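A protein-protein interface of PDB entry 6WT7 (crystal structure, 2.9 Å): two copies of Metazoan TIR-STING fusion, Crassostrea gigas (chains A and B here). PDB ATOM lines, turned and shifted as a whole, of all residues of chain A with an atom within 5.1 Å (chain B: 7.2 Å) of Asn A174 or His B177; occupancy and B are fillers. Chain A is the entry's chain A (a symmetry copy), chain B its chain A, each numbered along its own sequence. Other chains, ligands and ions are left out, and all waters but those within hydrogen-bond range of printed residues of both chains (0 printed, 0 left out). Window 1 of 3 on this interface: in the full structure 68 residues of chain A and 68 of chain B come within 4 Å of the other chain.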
ATOM      1  N   ASP A 110      23.181   1.165  21.582  1.00  0.00           N
ATOM      2  CA  ASP A 110      23.254  -0.114  22.269  1.00  0.00           C
ATOM      3  C   ASP A 110      22.561  -1.189  21.444  1.00  0.00           C
ATOM      4  O   ASP A 110      21.663  -0.905  20.646  1.00  0.00           O
ATOM      5  CB  ASP A 110      22.612  -0.014  23.656  1.00  0.00           C
ATOM      6  CG  ASP A 110      22.957  -1.191  24.555  1.00  0.00           C
ATOM      7  OD1 ASP A 110      22.929  -2.345  24.081  1.00  0.00           O
ATOM      8  OD2 ASP A 110      23.255  -0.958  25.744  1.00  0.00           O
ATOM      9  N   ASP A 111      22.994  -2.436  21.636  1.00  0.00           N
ATOM     10  CA  ASP A 111      22.330  -3.553  20.973  1.00  0.00           C
ATOM     11  C   ASP A 111      20.916  -3.738  21.502  1.00  0.00           C
ATOM     12  O   ASP A 111      19.989  -4.014  20.733  1.00  0.00           O
ATOM     13  CB  ASP A 111      23.137  -4.836  21.162  1.00  0.00           C
ATOM     14  CG  ASP A 111      24.626  -4.599  21.080  1.00  0.00           C
ATOM     15  OD1 ASP A 111      25.041  -3.674  20.351  1.00  0.00           O
ATOM     16  OD2 ASP A 111      25.382  -5.336  21.750  1.00  0.00           O
ATOM     17  N   SER A 112      20.735  -3.592  22.813  1.00  0.00           N
ATOM     18  CA  SER A 112      19.423  -3.727  23.428  1.00  0.00           C
ATOM     19  C   SER A 112      18.483  -2.643  22.919  1.00  0.00           C
ATOM     20  O   SER A 112      18.672  -1.458  23.216  1.00  0.00           O
ATOM     21  CB  SER A 112      19.537  -3.667  24.952  1.00  0.00           C
ATOM     22  OG  SER A 112      18.275  -3.858  25.565  1.00  0.00           O
ATOM     23  N   PRO A 171      18.306  -3.593  30.906  1.00  0.00           N
ATOM     24  CA  PRO A 171      18.122  -4.058  29.529  1.00  0.00           C
ATOM     25  C   PRO A 171      19.176  -5.078  29.133  1.00  0.00           C
ATOM     26  O   PRO A 171      20.335  -5.015  29.550  1.00  0.00           O
ATOM     27  CB  PRO A 171      18.259  -2.772  28.706  1.00  0.00           C
ATOM     28  CG  PRO A 171      19.182  -1.927  29.523  1.00  0.00           C
ATOM     29  CD  PRO A 171      18.859  -2.229  30.963  1.00  0.00           C
ATOM     30  N   VAL A 172      18.754  -6.027  28.305  1.00  0.00           N
ATOM     31  CA  VAL A 172      19.599  -7.134  27.874  1.00  0.00           C
ATOM     32  C   VAL A 172      19.673  -7.116  26.356  1.00  0.00           C
ATOM     33  O   VAL A 172      18.648  -7.256  25.677  1.00  0.00           O
ATOM     34  CB  VAL A 172      19.069  -8.485  28.375  1.00  0.00           C
ATOM     35  CG1 VAL A 172      19.912  -9.627  27.827  1.00  0.00           C
ATOM     36  CG2 VAL A 172      19.050  -8.513  29.892  1.00  0.00           C
ATOM     37  N   GLY A 173      20.883  -6.957  25.826  1.00  0.00           N
ATOM     38  CA  GLY A 173      21.100  -7.079  24.400  1.00  0.00           C
ATOM     39  C   GLY A 173      21.079  -8.530  23.967  1.00  0.00           C
ATOM     40  O   GLY A 173      20.419  -9.359  24.600  1.00  0.00           O
ATOM     41  N   ASN A 174      21.796  -8.861  22.901  1.00  0.00           N
ATOM     42  CA  ASN A 174      21.863 -10.234  22.426  1.00  0.00           C
ATOM     43  C   ASN A 174      23.175 -10.861  22.876  1.00  0.00           C
ATOM     44  O   ASN A 174      24.249 -10.280  22.684  1.00  0.00           O
ATOM     45  CB  ASN A 174      21.727 -10.299  20.906  1.00  0.00           C
ATOM     46  CG  ASN A 174      21.178 -11.628  20.437  1.00  0.00           C
ATOM     47  OD1 ASN A 174      21.672 -12.689  20.822  1.00  0.00           O
ATOM     48  ND2 ASN A 174      20.145 -11.579  19.605  1.00  0.00           N
ATOM     49  N   LEU A 175      23.080 -12.048  23.473  1.00  0.00           N
ATOM     50  CA  LEU A 175      24.216 -12.718  24.089  1.00  0.00           C
ATOM     51  C   LEU A 175      24.826 -13.803  23.212  1.00  0.00           C
ATOM     52  O   LEU A 175      25.902 -14.311  23.546  1.00  0.00           O
ATOM     53  CB  LEU A 175      23.787 -13.336  25.426  1.00  0.00           C
ATOM     54  CG  LEU A 175      23.017 -12.414  26.373  1.00  0.00           C
ATOM     55  CD1 LEU A 175      22.256 -13.217  27.418  1.00  0.00           C
ATOM     56  CD2 LEU A 175      23.962 -11.431  27.041  1.00  0.00           C
ATOM     57  N   ALA A 176      24.176 -14.157  22.101  1.00  0.00           N
ATOM     58  CA  ALA A 176      24.580 -15.332  21.334  1.00  0.00           C
ATOM     59  C   ALA A 176      26.005 -15.202  20.809  1.00  0.00           C
ATOM     60  O   ALA A 176      26.833 -16.101  20.995  1.00  0.00           O
ATOM     61  CB  ALA A 176      23.603 -15.560  20.182  1.00  0.00           C
ATOM     62  N   HIS A 177      26.312 -14.085  20.146  1.00  0.00           N
ATOM     63  CA  HIS A 177      27.611 -13.957  19.491  1.00  0.00           C
ATOM     64  C   HIS A 177      28.736 -13.788  20.502  1.00  0.00           C
ATOM     65  O   HIS A 177      29.819 -14.359  20.330  1.00  0.00           O
ATOM     66  CB  HIS A 177      27.587 -12.793  18.503  1.00  0.00           C
ATOM     67  CG  HIS A 177      26.990 -13.146  17.178  1.00  0.00           C
ATOM     68  ND1 HIS A 177      27.757 -13.466  16.079  1.00  0.00           N
ATOM     69  CD2 HIS A 177      25.700 -13.244  16.778  1.00  0.00           C
ATOM     70  CE1 HIS A 177      26.966 -13.738  15.057  1.00  0.00           C
ATOM     71  NE2 HIS A 177      25.713 -13.612  15.454  1.00  0.00           N
ATOM     72  N   GLN A 305      17.542 -16.642  23.032  1.00  0.00           N
ATOM     73  CA  GLN A 305      18.970 -16.345  23.080  1.00  0.00           C
ATOM     74  C   GLN A 305      19.808 -17.616  23.094  1.00  0.00           C
ATOM     75  O   GLN A 305      20.902 -17.646  22.517  1.00  0.00           O
ATOM     76  CB  GLN A 305      19.286 -15.490  24.308  1.00  0.00           C
ATOM     77  CG  GLN A 305      18.505 -14.185  24.383  1.00  0.00           C
ATOM     78  CD  GLN A 305      19.304 -12.988  23.910  1.00  0.00           C
ATOM     79  OE1 GLN A 305      20.472 -12.829  24.261  1.00  0.00           O
ATOM     80  NE2 GLN A 305      18.675 -12.137  23.107  1.00  0.00           N
ATOM     81  N   ARG A 308      19.801 -18.996  19.370  1.00  0.00           N
ATOM     82  CA  ARG A 308      20.722 -18.206  18.561  1.00  0.00           C
ATOM     83  C   ARG A 308      22.169 -18.517  18.918  1.00  0.00           C
ATOM     84  O   ARG A 308      23.044 -18.498  18.046  1.00  0.00           O
ATOM     85  CB  ARG A 308      20.438 -16.714  18.743  1.00  0.00           C
ATOM     86  CG  ARG A 308      19.210 -16.212  18.003  1.00  0.00           C
ATOM     87  CD  ARG A 308      18.846 -14.799  18.434  1.00  0.00           C
ATOM     88  NE  ARG A 308      17.954 -14.149  17.478  1.00  0.00           N
ATOM     89  CZ  ARG A 308      17.286 -13.026  17.719  1.00  0.00           C
ATOM     90  NH1 ARG A 308      17.397 -12.423  18.895  1.00  0.00           N
ATOM     91  NH2 ARG A 308      16.499 -12.507  16.785  1.00  0.00           N
ATOM     92  N   LEU B 106      12.050 -15.524  15.652  1.00  0.00           N
ATOM     93  CA  LEU B 106      13.302 -14.859  15.990  1.00  0.00           C
ATOM     94  C   LEU B 106      14.487 -15.814  16.002  1.00  0.00           C
ATOM     95  O   LEU B 106      15.631 -15.361  15.898  1.00  0.00           O
ATOM     96  CB  LEU B 106      13.174 -14.170  17.349  1.00  0.00           C
ATOM     97  CG  LEU B 106      12.082 -13.103  17.449  1.00  0.00           C
ATOM     98  CD1 LEU B 106      11.971 -12.581  18.872  1.00  0.00           C
ATOM     99  CD2 LEU B 106      12.353 -11.964  16.478  1.00  0.00           C
ATOM    100  N   VAL B 109      16.538 -15.434  12.980  1.00  0.00           N
ATOM    101  CA  VAL B 109      17.083 -14.098  12.776  1.00  0.00           C
ATOM    102  C   VAL B 109      18.389 -13.995  13.550  1.00  0.00           C
ATOM    103  O   VAL B 109      18.402 -14.113  14.781  1.00  0.00           O
ATOM    104  CB  VAL B 109      16.092 -13.010  13.218  1.00  0.00           C
ATOM    105  CG1 VAL B 109      16.736 -11.637  13.131  1.00  0.00           C
ATOM    106  CG2 VAL B 109      14.832 -13.070  12.372  1.00  0.00           C
ATOM    107  N   ASP B 110      19.485 -13.779  12.831  1.00  0.00           N
ATOM    108  CA  ASP B 110      20.790 -13.606  13.447  1.00  0.00           C
ATOM    109  C   ASP B 110      21.000 -12.143  13.816  1.00  0.00           C
ATOM    110  O   ASP B 110      20.417 -11.240  13.211  1.00  0.00           O
ATOM    111  CB  ASP B 110      21.898 -14.079  12.501  1.00  0.00           C
ATOM    112  CG  ASP B 110      23.237 -14.252  13.198  1.00  0.00           C
ATOM    113  OD1 ASP B 110      23.619 -13.381  14.007  1.00  0.00           O
ATOM    114  OD2 ASP B 110      23.915 -15.267  12.932  1.00  0.00           O
ATOM    115  N   ASP B 111      21.839 -11.917  14.828  1.00  0.00           N
ATOM    116  CA  ASP B 111      22.190 -10.549  15.196  1.00  0.00           C
ATOM    117  C   ASP B 111      23.003  -9.881  14.096  1.00  0.00           C
ATOM    118  O   ASP B 111      22.800  -8.699  13.796  1.00  0.00           O
ATOM    119  CB  ASP B 111      22.971 -10.539  16.508  1.00  0.00           C
ATOM    120  CG  ASP B 111      22.444 -11.547  17.501  1.00  0.00           C
ATOM    121  OD1 ASP B 111      21.228 -11.829  17.473  1.00  0.00           O
ATOM    122  OD2 ASP B 111      23.249 -12.061  18.309  1.00  0.00           O
ATOM    123  N   ASN B 174      27.094  -8.744  17.404  1.00  0.00           N
ATOM    124  CA  ASN B 174      27.593  -7.824  18.415  1.00  0.00           C
ATOM    125  C   ASN B 174      28.046  -8.612  19.636  1.00  0.00           C
ATOM    126  O   ASN B 174      27.307  -9.462  20.145  1.00  0.00           O
ATOM    127  CB  ASN B 174      26.529  -6.798  18.798  1.00  0.00           C
ATOM    128  CG  ASN B 174      27.135  -5.514  19.322  1.00  0.00           C
ATOM    129  OD1 ASN B 174      27.987  -5.533  20.212  1.00  0.00           O
ATOM    130  ND2 ASN B 174      26.703  -4.389  18.766  1.00  0.00           N
ATOM    131  N   LEU B 175      29.261  -8.323  20.099  1.00  0.00           N
ATOM    132  CA  LEU B 175      29.902  -9.077  21.166  1.00  0.00           C
ATOM    133  C   LEU B 175      29.803  -8.404  22.527  1.00  0.00           C
ATOM    134  O   LEU B 175      30.145  -9.031  23.535  1.00  0.00           O
ATOM    135  CB  LEU B 175      31.381  -9.301  20.822  1.00  0.00           C
ATOM    136  CG  LEU B 175      31.668  -9.837  19.418  1.00  0.00           C
ATOM    137  CD1 LEU B 175      33.116  -9.584  19.023  1.00  0.00           C
ATOM    138  CD2 LEU B 175      31.344 -11.318  19.338  1.00  0.00           C
ATOM    139  N   ALA B 176      29.336  -7.154  22.581  1.00  0.00           N
ATOM    140  CA  ALA B 176      29.421  -6.370  23.810  1.00  0.00           C
ATOM    141  C   ALA B 176      28.645  -7.021  24.949  1.00  0.00           C
ATOM    142  O   ALA B 176      29.175  -7.210  26.049  1.00  0.00           O
ATOM    143  CB  ALA B 176      28.913  -4.951  23.556  1.00  0.00           C
ATOM    144  N   HIS B 177      27.379  -7.369  24.705  1.00  0.00           N
ATOM    145  CA  HIS B 177      26.535  -7.860  25.790  1.00  0.00           C
ATOM    146  C   HIS B 177      26.943  -9.259  26.231  1.00  0.00           C
ATOM    147  O   HIS B 177      26.946  -9.558  27.431  1.00  0.00           O
ATOM    148  CB  HIS B 177      25.068  -7.830  25.367  1.00  0.00           C
ATOM    149  CG  HIS B 177      24.429  -6.486  25.522  1.00  0.00           C
ATOM    150  ND1 HIS B 177      23.649  -6.156  26.609  1.00  0.00           N
ATOM    151  CD2 HIS B 177      24.467  -5.384  24.736  1.00  0.00           C
ATOM    152  CE1 HIS B 177      23.227  -4.911  26.482  1.00  0.00           C
ATOM    153  NE2 HIS B 177      23.709  -4.420  25.354  1.00  0.00           N
ATOM    154  N   GLY B 178      27.287 -10.131  25.281  1.00  0.00           N
ATOM    155  CA  GLY B 178      27.749 -11.460  25.649  1.00  0.00           C
ATOM    156  C   GLY B 178      29.013 -11.424  26.487  1.00  0.00           C
ATOM    157  O   GLY B 178      29.130 -12.144  27.481  1.00  0.00           O
ATOM    158  N   PHE B 179      29.971 -10.579  26.103  1.00  0.00           N
ATOM    159  CA  PHE B 179      31.203 -10.448  26.873  1.00  0.00           C
ATOM    160  C   PHE B 179      30.926  -9.894  28.266  1.00  0.00           C
ATOM    161  O   PHE B 179      31.399 -10.438  29.270  1.00  0.00           O
ATOM    162  CB  PHE B 179      32.192  -9.545  26.135  1.00  0.00           C
ATOM    163  CG  PHE B 179      32.804 -10.167  24.913  1.00  0.00           C
ATOM    164  CD1 PHE B 179      32.636 -11.514  24.637  1.00  0.00           C
ATOM    165  CD2 PHE B 179      33.563  -9.399  24.045  1.00  0.00           C
ATOM    166  CE1 PHE B 179      33.209 -12.080  23.512  1.00  0.00           C
ATOM    167  CE2 PHE B 179      34.137  -9.959  22.921  1.00  0.00           C
ATOM    168  CZ  PHE B 179      33.959 -11.300  22.654  1.00  0.00           C
ATOM    169  N   ALA B 180      30.153  -8.807  28.345  1.00  0.00           N
ATOM    170  CA  ALA B 180      29.980  -8.102  29.612  1.00  0.00           C
ATOM    171  C   ALA B 180      29.198  -8.940  30.616  1.00  0.00           C
ATOM    172  O   ALA B 180      29.613  -9.088  31.772  1.00  0.00           O
ATOM    173  CB  ALA B 180      29.290  -6.761  29.376  1.00  0.00           C
ATOM    174  N   TRP B 181      28.052  -9.487  30.200  1.00  0.00           N
ATOM    175  CA  TRP B 181      27.248 -10.287  31.120  1.00  0.00           C
ATOM    176  C   TRP B 181      27.990 -11.545  31.551  1.00  0.00           C
ATOM    177  O   TRP B 181      27.949 -11.927  32.725  1.00  0.00           O
ATOM    178  CB  TRP B 181      25.909 -10.647  30.479  1.00  0.00           C
ATOM    179  CG  TRP B 181      24.948  -9.503  30.399  1.00  0.00           C
ATOM    180  CD1 TRP B 181      24.583  -8.813  29.280  1.00  0.00           C
ATOM    181  CD2 TRP B 181      24.227  -8.911  31.487  1.00  0.00           C
ATOM    182  NE1 TRP B 181      23.678  -7.830  29.602  1.00  0.00           N
ATOM    183  CE2 TRP B 181      23.444  -7.868  30.951  1.00  0.00           C
ATOM    184  CE3 TRP B 181      24.168  -9.161  32.862  1.00  0.00           C
ATOM    185  CZ2 TRP B 181      22.613  -7.078  31.741  1.00  0.00           C
ATOM    186  CZ3 TRP B 181      23.343  -8.374  33.644  1.00  0.00           C
ATOM    187  CH2 TRP B 181      22.577  -7.346  33.082  1.00  0.00           C
ATOM    188  N   GLY B 182      28.676 -12.201  30.614  1.00  0.00           N
ATOM    189  CA  GLY B 182      29.438 -13.385  30.970  1.00  0.00           C
ATOM    190  C   GLY B 182      30.589 -13.074  31.907  1.00  0.00           C
ATOM    191  O   GLY B 182      30.841 -13.810  32.863  1.00  0.00           O
ATOM    192  N   TYR B 183      31.298 -11.972  31.649  1.00  0.00           N
ATOM    193  CA  TYR B 183      32.412 -11.585  32.508  1.00  0.00           C
ATOM    194  C   TYR B 183      31.941 -11.263  33.921  1.00  0.00           C
ATOM    195  O   TYR B 183      32.667 -11.515  34.891  1.00  0.00           O
ATOM    196  CB  TYR B 183      33.145 -10.392  31.894  1.00  0.00           C
ATOM    197  CG  TYR B 183      34.484 -10.082  32.520  1.00  0.00           C
ATOM    198  CD1 TYR B 183      35.493 -11.034  32.555  1.00  0.00           C
ATOM    199  CD2 TYR B 183      34.749  -8.828  33.055  1.00  0.00           C
ATOM    200  CE1 TYR B 183      36.722 -10.754  33.121  1.00  0.00           C
ATOM    201  CE2 TYR B 183      35.978  -8.537  33.623  1.00  0.00           C
ATOM    202  CZ  TYR B 183      36.960  -9.504  33.652  1.00  0.00           C
ATOM    203  OH  TYR B 183      38.184  -9.223  34.214  1.00  0.00           O
ATOM    204  N   GLN B 305      33.008  -2.294  18.846  1.00  0.00           N
ATOM    205  CA  GLN B 305      32.553  -3.371  19.719  1.00  0.00           C
ATOM    206  C   GLN B 305      33.189  -3.280  21.100  1.00  0.00           C
ATOM    207  O   GLN B 305      32.545  -3.613  22.102  1.00  0.00           O
ATOM    208  CB  GLN B 305      32.862  -4.727  19.082  1.00  0.00           C
ATOM    209  CG  GLN B 305      32.260  -4.923  17.698  1.00  0.00           C
ATOM    210  CD  GLN B 305      30.982  -5.735  17.717  1.00  0.00           C
ATOM    211  OE1 GLN B 305      30.895  -6.761  18.389  1.00  0.00           O
ATOM    212  NE2 GLN B 305      29.979  -5.279  16.974  1.00  0.00           N
ATOM    213  N   ARG B 308      31.284  -0.369  23.013  1.00  0.00           N
ATOM    214  CA  ARG B 308      29.987  -0.857  23.466  1.00  0.00           C
ATOM    215  C   ARG B 308      30.142  -1.831  24.625  1.00  0.00           C
ATOM    216  O   ARG B 308      29.294  -1.870  25.524  1.00  0.00           O
ATOM    217  CB  ARG B 308      29.241  -1.522  22.309  1.00  0.00           C
ATOM    218  CG  ARG B 308      28.632  -0.553  21.310  1.00  0.00           C
ATOM    219  CD  ARG B 308      28.139  -1.278  20.068  1.00  0.00           C
ATOM    220  NE  ARG B 308      27.205  -0.464  19.294  1.00  0.00           N
ATOM    221  CZ  ARG B 308      26.817  -0.741  18.054  1.00  0.00           C
ATOM    222  NH1 ARG B 308      27.290  -1.812  17.430  1.00  0.00           N
ATOM    223  NH2 ARG B 308      25.960   0.058  17.431  1.00  0.00           N
ATOM    224  N   PHE B 309      31.221  -2.618  24.623  1.00  0.00           N
ATOM    225  CA  PHE B 309      31.499  -3.509  25.745  1.00  0.00           C
ATOM    226  C   PHE B 309      31.866  -2.723  26.996  1.00  0.00           C
ATOM    227  O   PHE B 309      31.434  -3.069  28.101  1.00  0.00           O
ATOM    228  CB  PHE B 309      32.618  -4.481  25.373  1.00  0.00           C
ATOM    229  CG  PHE B 309      33.237  -5.174  26.554  1.00  0.00           C
ATOM    230  CD1 PHE B 309      32.612  -6.260  27.140  1.00  0.00           C
ATOM    231  CD2 PHE B 309      34.445  -4.742  27.076  1.00  0.00           C
ATOM    232  CE1 PHE B 309      33.178  -6.903  28.226  1.00  0.00           C
ATOM    233  CE2 PHE B 309      35.013  -5.379  28.163  1.00  0.00           C
ATOM    234  CZ  PHE B 309      34.379  -6.462  28.736  1.00  0.00           C
ATOM    235  N   THR B 312      28.605  -1.204  28.399  1.00  0.00           N
ATOM    236  CA  THR B 312      27.707  -2.215  28.947  1.00  0.00           C
ATOM    237  C   THR B 312      28.238  -2.781  30.258  1.00  0.00           C
ATOM    238  O   THR B 312      27.484  -2.932  31.226  1.00  0.00           O
ATOM    239  CB  THR B 312      27.492  -3.332  27.926  1.00  0.00           C
ATOM    240  OG1 THR B 312      26.878  -2.789  26.752  1.00  0.00           O
ATOM    241  CG2 THR B 312      26.595  -4.416  28.501  1.00  0.00           C
ATOM    242  N   ARG B 315      27.881  -0.214  32.945  1.00  0.00           N
ATOM    243  CA  ARG B 315      26.482  -0.101  33.343  1.00  0.00           C
ATOM    244  C   ARG B 315      26.075  -1.257  34.247  1.00  0.00           C
ATOM    245  O   ARG B 315      25.321  -1.066  35.209  1.00  0.00           O
ATOM    246  CB  ARG B 315      25.580  -0.033  32.110  1.00  0.00           C
ATOM    247  CG  ARG B 315      25.432   1.367  31.534  1.00  0.00           C
ATOM    248  CD  ARG B 315      24.380   1.432  30.435  1.00  0.00           C
ATOM    249  NE  ARG B 315      24.834   0.830  29.184  1.00  0.00           N
ATOM    250  CZ  ARG B 315      24.410  -0.340  28.715  1.00  0.00           C
ATOM    251  NH1 ARG B 315      23.508  -1.042  29.390  1.00  0.00           N
ATOM    252  NH2 ARG B 315      24.883  -0.806  27.567  1.00  0.00           N
ATOM    253  N   ILE B 316      26.569  -2.465  33.958  1.00  0.00           N
ATOM    254  CA  ILE B 316      26.270  -3.615  34.806  1.00  0.00           C
ATOM    255  C   ILE B 316      26.882  -3.432  36.188  1.00  0.00           C
ATOM    256  O   ILE B 316      26.248  -3.730  37.209  1.00  0.00           O
ATOM    257  CB  ILE B 316      26.762  -4.914  34.139  1.00  0.00           C
ATOM    258  CG1 ILE B 316      25.984  -5.187  32.852  1.00  0.00           C
ATOM    259  CG2 ILE B 316      26.634  -6.094  35.095  1.00  0.00           C
ATOM    260  CD1 ILE B 316      26.503  -6.371  32.074  1.00  0.00           C
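Among the printed residues, merely in contact across the chains: Asp A111 with Ala B176 (3.98 Å), Asp A111 with His B177 (3.1 Å), Asp A111 with Arg B308 (3.9 Å), Ser A112 with His B177 (3.998 Å), Pro A171 with Trp B181 (3.8 Å), Asn A174 with His B177 (3.7 Å), Asn A174 with Gly B178 (3.9995 Å), Leu A175 with His B177 (3.5 Å), Leu A175 with Gly B178 (3.98 Å), Leu A175 with Trp B181 (3.5 Å), Ala A176 with Asp B111 (3.98 Å), His A177 with Asp B111 (3.1 Å), His A177 with Asn B174 (3.7 Å), His A177 with Leu B175 (3.5 Å) and Arg A308 with Asp B111 (3.9 Å).
Printed residues of chain B within 4 Å of Asn A174: Asp B111, His B177 and Gly B178. Of the printed residues of chain A, His B177 touches Asp A110 (2.6 Å), Asp A111 (3.1 Å), Ser A112 (3.998 Å), Gly A173 (3.0 Å), Asn A174 (3.7 Å) and Leu A175 (3.5 Å). Printed residues of chain B within 4 Å of Gly A173: His B177 (3.0 Å). Of the printed residues of chain A, Asn B174 touches Asp A111 (2.4 Å) and His A177 (3.7 Å). Printed residues of chain B within 4 Å of His A177: Asp B110 (2.6 Å), Asp B111 (3.1 Å), Asn B174 (3.7 Å) and Leu B175 (3.5 Å). Of the printed residues of chain B, Pro A171 touches Trp B181. Thr B312 touches none of the printed residues of chain A. Phe B309 touches none of the printed residues of chain A. The nearest printed residue of chain A that does not touch His B177 is Val A172 (4.1 Å). The nearest printed residue of chain A that does not touch Leu B106 is Asn A174 (7.0 Å).
The backbone carbonyl oxygen (O) of Leu B106 lies within hydrogen-bond range of the guanidinium group (NE) of Arg A308 (3.1 Å). O of Val B109 lies within hydrogen-bond range of NE of Arg A308, 2.7 Å away. NE2 of His A177 sits at hydrogen-bond distance from OD1 of Asp B110, at 2.6 Å. ND2 of Asn A174 is in hydrogen-bond range of OD1 of Asp B111 (2.4 Å). The side-chain amide nitrogen (ND2) of Asn B174 lies within hydrogen-bond range of the side-chain carboxylate (OD1) of Asp A111, 2.4 Å away. The side-chain carboxylate of Asp A110 sits at hydrogen-bond distance from a ring nitrogen (NE2) of His B177 (2.6 Å). ND1 of His B177 is in hydrogen-bond range of N of Gly A173, 3.0 Å away. NH2 of Arg B315 lies within salt-bridge range of OD2 of Asp A110, at 2.4 Å.
Hydrophobic or aromatic side chains of chain A that line the printed part of chain B: Leu A175, Ala A176 and His A177. Printed residues of chain B that touch a printed residue of chain A: Leu B106, Val B109, Asp B110, Asp B111, Asn B174, Leu B175, Ala B176, His B177, Gly B178, Trp B181, Arg B308 and Arg B315. Among the printed residues, 23 pairs touch across the chains. Among the printed residues, Asp or Glu carboxylates within 4 Å of a Lys or Arg side-chain nitrogen of the other chain: Asp A110 with Arg B315.
OD1 of Asn B174 is in hydrogen-bond range of N of Ala B176, at 3.2 Å. N of Leu B175 lies within hydrogen-bond range of OE1 of Gln B305 (2.8 Å). The side-chain hydroxyl of Ser A112 is in hydrogen-bond range of the backbone carbonyl oxygen of Val A172, 3.4 Å away. O of Gly A173 sits close to OE1 of Gln A305 (3.5 Å). N of Ala A176 sits at hydrogen-bond distance from OD1 of Asn A174 (3.2 Å). N of Leu A175 is in hydrogen-bond range of OE1 of Gln A305.
Asp A110 touches His B177, and with the chains exchanged His A177 touches Asp B110. Asp A111 touches Asn B174, and with the chains exchanged Asn A174 touches Asp B111. Asp A111 touches Ala B176, and with the chains exchanged Ala A176 touches Asp B111. Asn A174 touches His B177, and with the chains exchanged His A177 touches Asn B174. Positions printed for both chains: 110, 111, 174, 175, 176, 177, 305 and 308. Of the 23 pairs that touch across the chains among the printed residues, 14 have their exchanged pair printed and touching as well.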
